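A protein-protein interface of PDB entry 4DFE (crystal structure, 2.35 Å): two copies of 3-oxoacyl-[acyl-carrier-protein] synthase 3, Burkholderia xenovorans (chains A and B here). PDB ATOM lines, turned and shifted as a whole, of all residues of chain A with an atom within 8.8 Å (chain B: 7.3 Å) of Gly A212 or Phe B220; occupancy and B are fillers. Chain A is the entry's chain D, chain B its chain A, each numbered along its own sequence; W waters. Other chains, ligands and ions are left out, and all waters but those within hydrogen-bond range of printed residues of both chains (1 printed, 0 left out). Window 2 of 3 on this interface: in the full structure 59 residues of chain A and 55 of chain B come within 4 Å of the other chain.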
ATOM      1  N   VAL A 100      13.369 -21.222  -5.114  1.00  0.00           N
ATOM      2  CA  VAL A 100      14.425 -20.510  -5.841  1.00  0.00           C
ATOM      3  C   VAL A 100      15.339 -21.559  -6.454  1.00  0.00           C
ATOM      4  O   VAL A 100      15.690 -21.475  -7.625  1.00  0.00           O
ATOM      5  CB  VAL A 100      15.274 -19.599  -4.929  1.00  0.00           C
ATOM      6  CG1 VAL A 100      16.589 -19.254  -5.594  1.00  0.00           C
ATOM      7  CG2 VAL A 100      14.517 -18.328  -4.563  1.00  0.00           C
ATOM      8  N   PHE A 101      15.750 -22.519  -5.626  1.00  0.00           N
ATOM      9  CA  PHE A 101      16.347 -23.770  -6.088  1.00  0.00           C
ATOM     10  C   PHE A 101      16.254 -24.787  -4.980  1.00  0.00           C
ATOM     11  O   PHE A 101      16.015 -24.411  -3.820  1.00  0.00           O
ATOM     12  CB  PHE A 101      17.793 -23.580  -6.599  1.00  0.00           C
ATOM     13  CG  PHE A 101      18.859 -23.437  -5.527  1.00  0.00           C
ATOM     14  CD1 PHE A 101      19.390 -24.543  -4.908  1.00  0.00           C
ATOM     15  CD2 PHE A 101      19.448 -22.197  -5.284  1.00  0.00           C
ATOM     16  CE1 PHE A 101      20.422 -24.419  -3.999  1.00  0.00           C
ATOM     17  CE2 PHE A 101      20.503 -22.058  -4.384  1.00  0.00           C
ATOM     18  CZ  PHE A 101      20.984 -23.171  -3.733  1.00  0.00           C
ATOM     19  N   ASN A 209      12.051 -10.066  -7.487  1.00  0.00           N
ATOM     20  CA  ASN A 209      12.576 -11.343  -7.016  1.00  0.00           C
ATOM     21  C   ASN A 209      13.010 -11.187  -5.571  1.00  0.00           C
ATOM     22  O   ASN A 209      12.939 -10.087  -4.996  1.00  0.00           O
ATOM     23  CB  ASN A 209      13.762 -11.833  -7.896  1.00  0.00           C
ATOM     24  CG  ASN A 209      13.814 -13.364  -8.025  1.00  0.00           C
ATOM     25  OD1 ASN A 209      13.230 -14.068  -7.229  1.00  0.00           O
ATOM     26  ND2 ASN A 209      14.458 -13.863  -9.054  1.00  0.00           N
ATOM     27  N   VAL A 210      13.512 -12.257  -4.983  1.00  0.00           N
ATOM     28  CA  VAL A 210      13.913 -12.191  -3.602  1.00  0.00           C
ATOM     29  C   VAL A 210      15.339 -11.664  -3.458  1.00  0.00           C
ATOM     30  O   VAL A 210      16.205 -11.897  -4.293  1.00  0.00           O
ATOM     31  CB  VAL A 210      13.793 -13.535  -2.936  1.00  0.00           C
ATOM     32  CG1 VAL A 210      12.411 -14.077  -3.209  1.00  0.00           C
ATOM     33  CG2 VAL A 210      14.873 -14.463  -3.479  1.00  0.00           C
ATOM     34  N   ASN A 211      15.550 -10.943  -2.365  1.00  0.00           N
ATOM     35  CA  ASN A 211      16.805 -10.290  -2.098  1.00  0.00           C
ATOM     36  C   ASN A 211      16.928 -10.087  -0.587  1.00  0.00           C
ATOM     37  O   ASN A 211      16.115  -9.377   0.026  1.00  0.00           O
ATOM     38  CB  ASN A 211      16.851  -8.936  -2.826  1.00  0.00           C
ATOM     39  CG  ASN A 211      18.240  -8.304  -2.810  1.00  0.00           C
ATOM     40  OD1 ASN A 211      19.147  -8.828  -2.197  1.00  0.00           O
ATOM     41  ND2 ASN A 211      18.395  -7.156  -3.463  1.00  0.00           N
ATOM     42  N   GLY A 212      17.885 -10.766   0.027  1.00  0.00           N
ATOM     43  CA  GLY A 212      18.099 -10.661   1.458  1.00  0.00           C
ATOM     44  C   GLY A 212      16.852 -10.999   2.262  1.00  0.00           C
ATOM     45  O   GLY A 212      16.520 -10.271   3.203  1.00  0.00           O
ATOM     46  N   GLY A 213      16.155 -12.073   1.874  1.00  0.00           N
ATOM     47  CA  GLY A 213      15.023 -12.568   2.625  1.00  0.00           C
ATOM     48  C   GLY A 213      13.679 -11.954   2.266  1.00  0.00           C
ATOM     49  O   GLY A 213      12.657 -12.572   2.491  1.00  0.00           O
ATOM     50  N   VAL A 214      13.673 -10.737   1.732  1.00  0.00           N
ATOM     51  CA  VAL A 214      12.428 -10.040   1.359  1.00  0.00           C
ATOM     52  C   VAL A 214      12.279  -9.920  -0.161  1.00  0.00           C
ATOM     53  O   VAL A 214      13.242 -10.035  -0.886  1.00  0.00           O
ATOM     54  CB  VAL A 214      12.405  -8.611   1.948  1.00  0.00           C
ATOM     55  CG1 VAL A 214      12.688  -8.664   3.441  1.00  0.00           C
ATOM     56  CG2 VAL A 214      13.405  -7.672   1.242  1.00  0.00           C
ATOM     57  N   VAL A 215      11.073  -9.611  -0.620  1.00  0.00           N
ATOM     58  CA  VAL A 215      10.831  -9.282  -2.014  1.00  0.00           C
ATOM     59  C   VAL A 215      11.312  -7.877  -2.340  1.00  0.00           C
ATOM     60  O   VAL A 215      11.018  -6.949  -1.601  1.00  0.00           O
ATOM     61  CB  VAL A 215       9.329  -9.280  -2.305  1.00  0.00           C
ATOM     62  CG1 VAL A 215       9.072  -8.851  -3.744  1.00  0.00           C
ATOM     63  CG2 VAL A 215       8.745 -10.637  -2.023  1.00  0.00           C
ATOM     64  N   SER A 216      12.073  -7.717  -3.413  1.00  0.00           N
ATOM     65  CA  SER A 216      12.370  -6.373  -3.940  1.00  0.00           C
ATOM     66  C   SER A 216      11.721  -6.255  -5.317  1.00  0.00           C
ATOM     67  O   SER A 216      11.480  -7.270  -5.983  1.00  0.00           O
ATOM     68  CB  SER A 216      13.863  -6.129  -4.039  1.00  0.00           C
ATOM     69  OG  SER A 216      14.396  -6.914  -5.078  1.00  0.00           O
ATOM     70  N   SER B 158      24.775 -13.384  -3.523  1.00  0.00           N
ATOM     71  CA  SER B 158      24.662 -12.585  -2.304  1.00  0.00           C
ATOM     72  C   SER B 158      23.198 -12.272  -1.927  1.00  0.00           C
ATOM     73  O   SER B 158      22.922 -11.976  -0.771  1.00  0.00           O
ATOM     74  CB  SER B 158      25.439 -11.287  -2.455  1.00  0.00           C
ATOM     75  OG  SER B 158      25.167 -10.703  -3.720  1.00  0.00           O
ATOM     76  N   ARG B 159      22.273 -12.306  -2.894  1.00  0.00           N
ATOM     77  CA  ARG B 159      20.857 -11.997  -2.626  1.00  0.00           C
ATOM     78  C   ARG B 159      20.116 -13.102  -1.860  1.00  0.00           C
ATOM     79  O   ARG B 159      19.023 -12.876  -1.320  1.00  0.00           O
ATOM     80  CB  ARG B 159      20.097 -11.720  -3.937  1.00  0.00           C
ATOM     81  CG  ARG B 159      20.558 -10.476  -4.704  1.00  0.00           C
ATOM     82  CD  ARG B 159      19.876 -10.434  -6.068  1.00  0.00           C
ATOM     83  NE  ARG B 159      20.094  -9.195  -6.807  1.00  0.00           N
ATOM     84  CZ  ARG B 159      19.151  -8.314  -7.116  1.00  0.00           C
ATOM     85  NH1 ARG B 159      19.473  -7.175  -7.765  1.00  0.00           N
ATOM     86  NH2 ARG B 159      17.901  -8.521  -6.742  1.00  0.00           N
ATOM     87  N   ILE B 160      20.703 -14.289  -1.810  1.00  0.00           N
ATOM     88  CA  ILE B 160      20.049 -15.429  -1.186  1.00  0.00           C
ATOM     89  C   ILE B 160      20.901 -15.995  -0.049  1.00  0.00           C
ATOM     90  O   ILE B 160      20.685 -17.145   0.382  1.00  0.00           O
ATOM     91  CB  ILE B 160      19.717 -16.534  -2.237  1.00  0.00           C
ATOM     92  CG1 ILE B 160      20.992 -17.021  -2.935  1.00  0.00           C
ATOM     93  CG2 ILE B 160      18.738 -16.022  -3.298  1.00  0.00           C
ATOM     94  CD1 ILE B 160      20.760 -17.998  -4.064  1.00  0.00           C
ATOM     95  N   LEU B 161      21.890 -15.222   0.414  1.00  0.00           N
ATOM     96  CA  LEU B 161      22.749 -15.663   1.511  1.00  0.00           C
ATOM     97  C   LEU B 161      22.172 -15.197   2.832  1.00  0.00           C
ATOM     98  O   LEU B 161      21.765 -14.051   2.967  1.00  0.00           O
ATOM     99  CB  LEU B 161      24.178 -15.126   1.343  1.00  0.00           C
ATOM    100  CG  LEU B 161      25.094 -15.782   0.285  1.00  0.00           C
ATOM    101  CD1 LEU B 161      26.551 -15.330   0.475  1.00  0.00           C
ATOM    102  CD2 LEU B 161      25.025 -17.308   0.326  1.00  0.00           C
ATOM    103  N   ASP B 162      22.119 -16.096   3.797  1.00  0.00           N
ATOM    104  CA  ASP B 162      21.888 -15.699   5.192  1.00  0.00           C
ATOM    105  C   ASP B 162      23.231 -15.333   5.877  1.00  0.00           C
ATOM    106  O   ASP B 162      24.019 -16.215   6.198  1.00  0.00           O
ATOM    107  CB  ASP B 162      21.193 -16.841   5.951  1.00  0.00           C
ATOM    108  CG  ASP B 162      20.796 -16.467   7.377  1.00  0.00           C
ATOM    109  OD1 ASP B 162      21.125 -15.347   7.838  1.00  0.00           O
ATOM    110  OD2 ASP B 162      20.152 -17.313   8.046  1.00  0.00           O
ATOM    111  N   PHE B 163      23.454 -14.056   6.142  1.00  0.00           N
ATOM    112  CA  PHE B 163      24.686 -13.651   6.816  1.00  0.00           C
ATOM    113  C   PHE B 163      24.755 -13.956   8.348  1.00  0.00           C
ATOM    114  O   PHE B 163      25.778 -13.672   9.001  1.00  0.00           O
ATOM    115  CB  PHE B 163      25.017 -12.189   6.484  1.00  0.00           C
ATOM    116  CG  PHE B 163      25.370 -11.992   5.046  1.00  0.00           C
ATOM    117  CD1 PHE B 163      26.658 -12.254   4.596  1.00  0.00           C
ATOM    118  CD2 PHE B 163      24.395 -11.664   4.115  1.00  0.00           C
ATOM    119  CE1 PHE B 163      26.987 -12.117   3.246  1.00  0.00           C
ATOM    120  CE2 PHE B 163      24.716 -11.522   2.767  1.00  0.00           C
ATOM    121  CZ  PHE B 163      26.016 -11.743   2.334  1.00  0.00           C
ATOM    122  N   THR B 168      27.615 -21.151   5.226  1.00  0.00           N
ATOM    123  CA  THR B 168      27.366 -20.890   3.821  1.00  0.00           C
ATOM    124  C   THR B 168      27.718 -19.461   3.369  1.00  0.00           C
ATOM    125  O   THR B 168      28.007 -19.252   2.211  1.00  0.00           O
ATOM    126  CB  THR B 168      25.885 -21.131   3.507  1.00  0.00           C
ATOM    127  OG1 THR B 168      25.097 -20.271   4.325  1.00  0.00           O
ATOM    128  CG2 THR B 168      25.479 -22.616   3.762  1.00  0.00           C
ATOM    129  N   CYS B 205      19.673 -26.376  -0.823  1.00  0.00           N
ATOM    130  CA  CYS B 205      18.431 -25.775  -1.269  1.00  0.00           C
ATOM    131  C   CYS B 205      18.266 -24.363  -0.754  1.00  0.00           C
ATOM    132  O   CYS B 205      18.769 -24.019   0.317  1.00  0.00           O
ATOM    133  CB  CYS B 205      17.224 -26.617  -0.828  1.00  0.00           C
ATOM    134  SG  CYS B 205      17.037 -26.872   0.955  1.00  0.00           S
ATOM    135  N   THR B 206      17.543 -23.550  -1.523  1.00  0.00           N
ATOM    136  CA  THR B 206      17.046 -22.265  -1.051  1.00  0.00           C
ATOM    137  C   THR B 206      15.507 -22.355  -1.059  1.00  0.00           C
ATOM    138  O   THR B 206      14.854 -21.969  -2.044  1.00  0.00           O
ATOM    139  CB  THR B 206      17.587 -21.129  -1.916  1.00  0.00           C
ATOM    140  OG1 THR B 206      19.015 -21.167  -1.902  1.00  0.00           O
ATOM    141  CG2 THR B 206      17.142 -19.781  -1.412  1.00  0.00           C
ATOM    142  N   PRO B 207      14.924 -22.931   0.029  1.00  0.00           N
ATOM    143  CA  PRO B 207      13.595 -23.495  -0.026  1.00  0.00           C
ATOM    144  C   PRO B 207      12.488 -22.459   0.172  1.00  0.00           C
ATOM    145  O   PRO B 207      11.751 -22.509   1.158  1.00  0.00           O
ATOM    146  CB  PRO B 207      13.616 -24.531   1.112  1.00  0.00           C
ATOM    147  CG  PRO B 207      14.505 -23.928   2.124  1.00  0.00           C
ATOM    148  CD  PRO B 207      15.514 -23.075   1.366  1.00  0.00           C
ATOM    149  N   GLY B 208      12.378 -21.520  -0.760  1.00  0.00           N
ATOM    150  CA  GLY B 208      11.242 -20.613  -0.788  1.00  0.00           C
ATOM    151  C   GLY B 208      11.069 -19.959  -2.144  1.00  0.00           C
ATOM    152  O   GLY B 208      11.852 -20.188  -3.058  1.00  0.00           O
ATOM    153  N   VAL B 215       7.473 -13.235   0.538  1.00  0.00           N
ATOM    154  CA  VAL B 215       8.241 -14.479   0.504  1.00  0.00           C
ATOM    155  C   VAL B 215       7.535 -15.518   1.371  1.00  0.00           C
ATOM    156  O   VAL B 215       7.204 -15.228   2.515  1.00  0.00           O
ATOM    157  CB  VAL B 215       9.650 -14.290   1.101  1.00  0.00           C
ATOM    158  CG1 VAL B 215      10.366 -15.617   1.208  1.00  0.00           C
ATOM    159  CG2 VAL B 215      10.477 -13.280   0.309  1.00  0.00           C
ATOM    160  N   GLY B 217       8.179 -19.717   2.762  1.00  0.00           N
ATOM    161  CA  GLY B 217       9.339 -20.584   3.011  1.00  0.00           C
ATOM    162  C   GLY B 217      10.532 -19.754   3.452  1.00  0.00           C
ATOM    163  O   GLY B 217      10.366 -18.752   4.138  1.00  0.00           O
ATOM    164  N   SER B 218      11.741 -20.180   3.100  1.00  0.00           N
ATOM    165  CA  SER B 218      12.944 -19.359   3.332  1.00  0.00           C
ATOM    166  C   SER B 218      13.620 -19.103   2.016  1.00  0.00           C
ATOM    167  O   SER B 218      13.920 -20.035   1.257  1.00  0.00           O
ATOM    168  CB  SER B 218      13.922 -20.021   4.301  1.00  0.00           C
ATOM    169  OG  SER B 218      14.487 -19.043   5.174  1.00  0.00           O
ATOM    170  N   ALA B 219      13.846 -17.828   1.740  1.00  0.00           N
ATOM    171  CA  ALA B 219      14.558 -17.422   0.545  1.00  0.00           C
ATOM    172  C   ALA B 219      16.065 -17.245   0.845  1.00  0.00           C
ATOM    173  O   ALA B 219      16.721 -16.357   0.302  1.00  0.00           O
ATOM    174  CB  ALA B 219      13.942 -16.146  -0.025  1.00  0.00           C
ATOM    175  N   PHE B 220      16.596 -18.123   1.699  1.00  0.00           N
ATOM    176  CA  PHE B 220      18.018 -18.156   2.049  1.00  0.00           C
ATOM    177  C   PHE B 220      18.574 -19.549   1.785  1.00  0.00           C
ATOM    178  O   PHE B 220      17.905 -20.564   2.030  1.00  0.00           O
ATOM    179  CB  PHE B 220      18.260 -17.808   3.531  1.00  0.00           C
ATOM    180  CG  PHE B 220      18.074 -16.340   3.874  1.00  0.00           C
ATOM    181  CD1 PHE B 220      18.679 -15.330   3.107  1.00  0.00           C
ATOM    182  CD2 PHE B 220      17.340 -15.969   5.015  1.00  0.00           C
ATOM    183  CE1 PHE B 220      18.515 -13.996   3.440  1.00  0.00           C
ATOM    184  CE2 PHE B 220      17.176 -14.628   5.348  1.00  0.00           C
ATOM    185  CZ  PHE B 220      17.768 -13.642   4.561  1.00  0.00           C
ATOM    186  N   LEU B 221      19.814 -19.595   1.308  1.00  0.00           N
ATOM    187  CA  LEU B 221      20.471 -20.854   0.987  1.00  0.00           C
ATOM    188  C   LEU B 221      20.846 -21.614   2.261  1.00  0.00           C
ATOM    189  O   LEU B 221      21.441 -21.051   3.154  1.00  0.00           O
ATOM    190  CB  LEU B 221      21.716 -20.579   0.147  1.00  0.00           C
ATOM    191  CG  LEU B 221      22.464 -21.772  -0.456  1.00  0.00           C
ATOM    192  CD1 LEU B 221      23.260 -21.319  -1.678  1.00  0.00           C
ATOM    193  CD2 LEU B 221      23.356 -22.465   0.562  1.00  0.00           C
ATOM    194  N   HIS B 222      20.502 -22.903   2.304  1.00  0.00           N
ATOM    195  CA  HIS B 222      20.870 -23.791   3.390  1.00  0.00           C
ATOM    196  C   HIS B 222      21.531 -25.046   2.830  1.00  0.00           C
ATOM    197  O   HIS B 222      21.321 -25.423   1.678  1.00  0.00           O
ATOM    198  CB  HIS B 222      19.615 -24.046   4.237  1.00  0.00           C
ATOM    199  CG  HIS B 222      19.266 -25.467   4.438  1.00  0.00           C
ATOM    200  ND1 HIS B 222      20.085 -26.351   5.025  1.00  0.00           N
ATOM    201  CD2 HIS B 222      18.086 -26.145   4.147  1.00  0.00           C
ATOM    202  CE1 HIS B 222      19.468 -27.549   5.077  1.00  0.00           C
ATOM    203  NE2 HIS B 222      18.248 -27.415   4.540  1.00  0.00           N
ATOM    204  N   MET B 223      22.389 -25.675   3.616  1.00  0.00           N
ATOM    205  CA  MET B 223      23.286 -26.698   3.092  1.00  0.00           C
ATOM    206  C   MET B 223      23.787 -27.597   4.217  1.00  0.00           C
ATOM    207  O   MET B 223      24.088 -27.127   5.314  1.00  0.00           O
ATOM    208  CB  MET B 223      24.459 -25.990   2.410  1.00  0.00           C
ATOM    209  CG  MET B 223      25.500 -26.882   1.759  1.00  0.00           C
ATOM    210  SD  MET B 223      26.911 -25.903   1.205  1.00  0.00           S
ATOM    211  CE  MET B 223      28.012 -26.088   2.615  1.00  0.00           C
HETATM  212  O   HOH W   1      16.390 -13.810  -0.894  1.00  0.00           O
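The backbone NH of Leu B221 is in hydrogen-bond range of the backbone carbonyl oxygen of Ile B160, 2.8 Å away. N of His B222 lies within hydrogen-bond range of O of Cys B205. N of Gly B208 is in hydrogen-bond range of O of Ser B218.
Gly A212 touches just these residues of chain B: Arg B159 and Phe B220. Phe B220 touches just these residues of chain A: Gly A212 and Gly A213. Ala B219 touches just one residue of chain A: Val A210. Printed residues of chain B within 4 Å of Val A214: Val B215. Printed residues of chain A within 4 Å of Val B215: Gly A213 (3.2 Å), Val A214 (3.8 Å) and Val A215 (3.8 Å). Printed residues of chain A within 4 Å of Gly B208: Val A100. Ile B160 touches none of the printed residues of chain A. His B222 touches none of the printed residues of chain A. The nearest residue of chain B that does not touch Gly A212 is Ile B160 (4.9 Å). The nearest residue of chain A that does not touch Phe B220 is Val A214 (5.8 Å).
Val B215 touches its own counterpart, Val A215.
Of the 10 printed residues of chain A, 8 touch a printed residue of chain B.
N of Gly A212 is in hydrogen-bond range of O of Arg B159. The backbone carbonyl oxygen (O) of Thr B206 lies within hydrogen-bond range of the backbone NH (N) of Val A100 (3.5 Å). The backbone carbonyl oxygen of Phe A101 sits at hydrogen-bond distance from the backbone NH of Thr B206 (2.9 Å). The backbone carbonyl oxygen (O) of Gly B208 lies within hydrogen-bond range of the backbone NH (N) of Val A100 (2.8 Å).
Water W1 lies within hydrogen-bond range of O of Arg B159, O of Ala B219, N of Gly A213 and N of Asn A211.
Phe A101 touches Cys B205. CZ of Phe A101 touches CD1 of Leu B221 (3.6 Å). Arg B159 touches Val A210 (CB to O, 3.9 Å). CB of Val A210 touches CB of Ala B219, at 3.9 Å. Asn A211 touches Arg B159. Gly A212 touches Phe B220 (C to CZ, 3.6 Å). CG2 of Val B215 touches O of Gly A213, 3.2 Å away. Gly A213 touches Phe B220 (N to CE1, 3.4 Å). Val A214 touches Val B215 (C to CG2, 3.8 Å). Val B215 touches Val A215 (CG2 to N, 3.8 Å).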
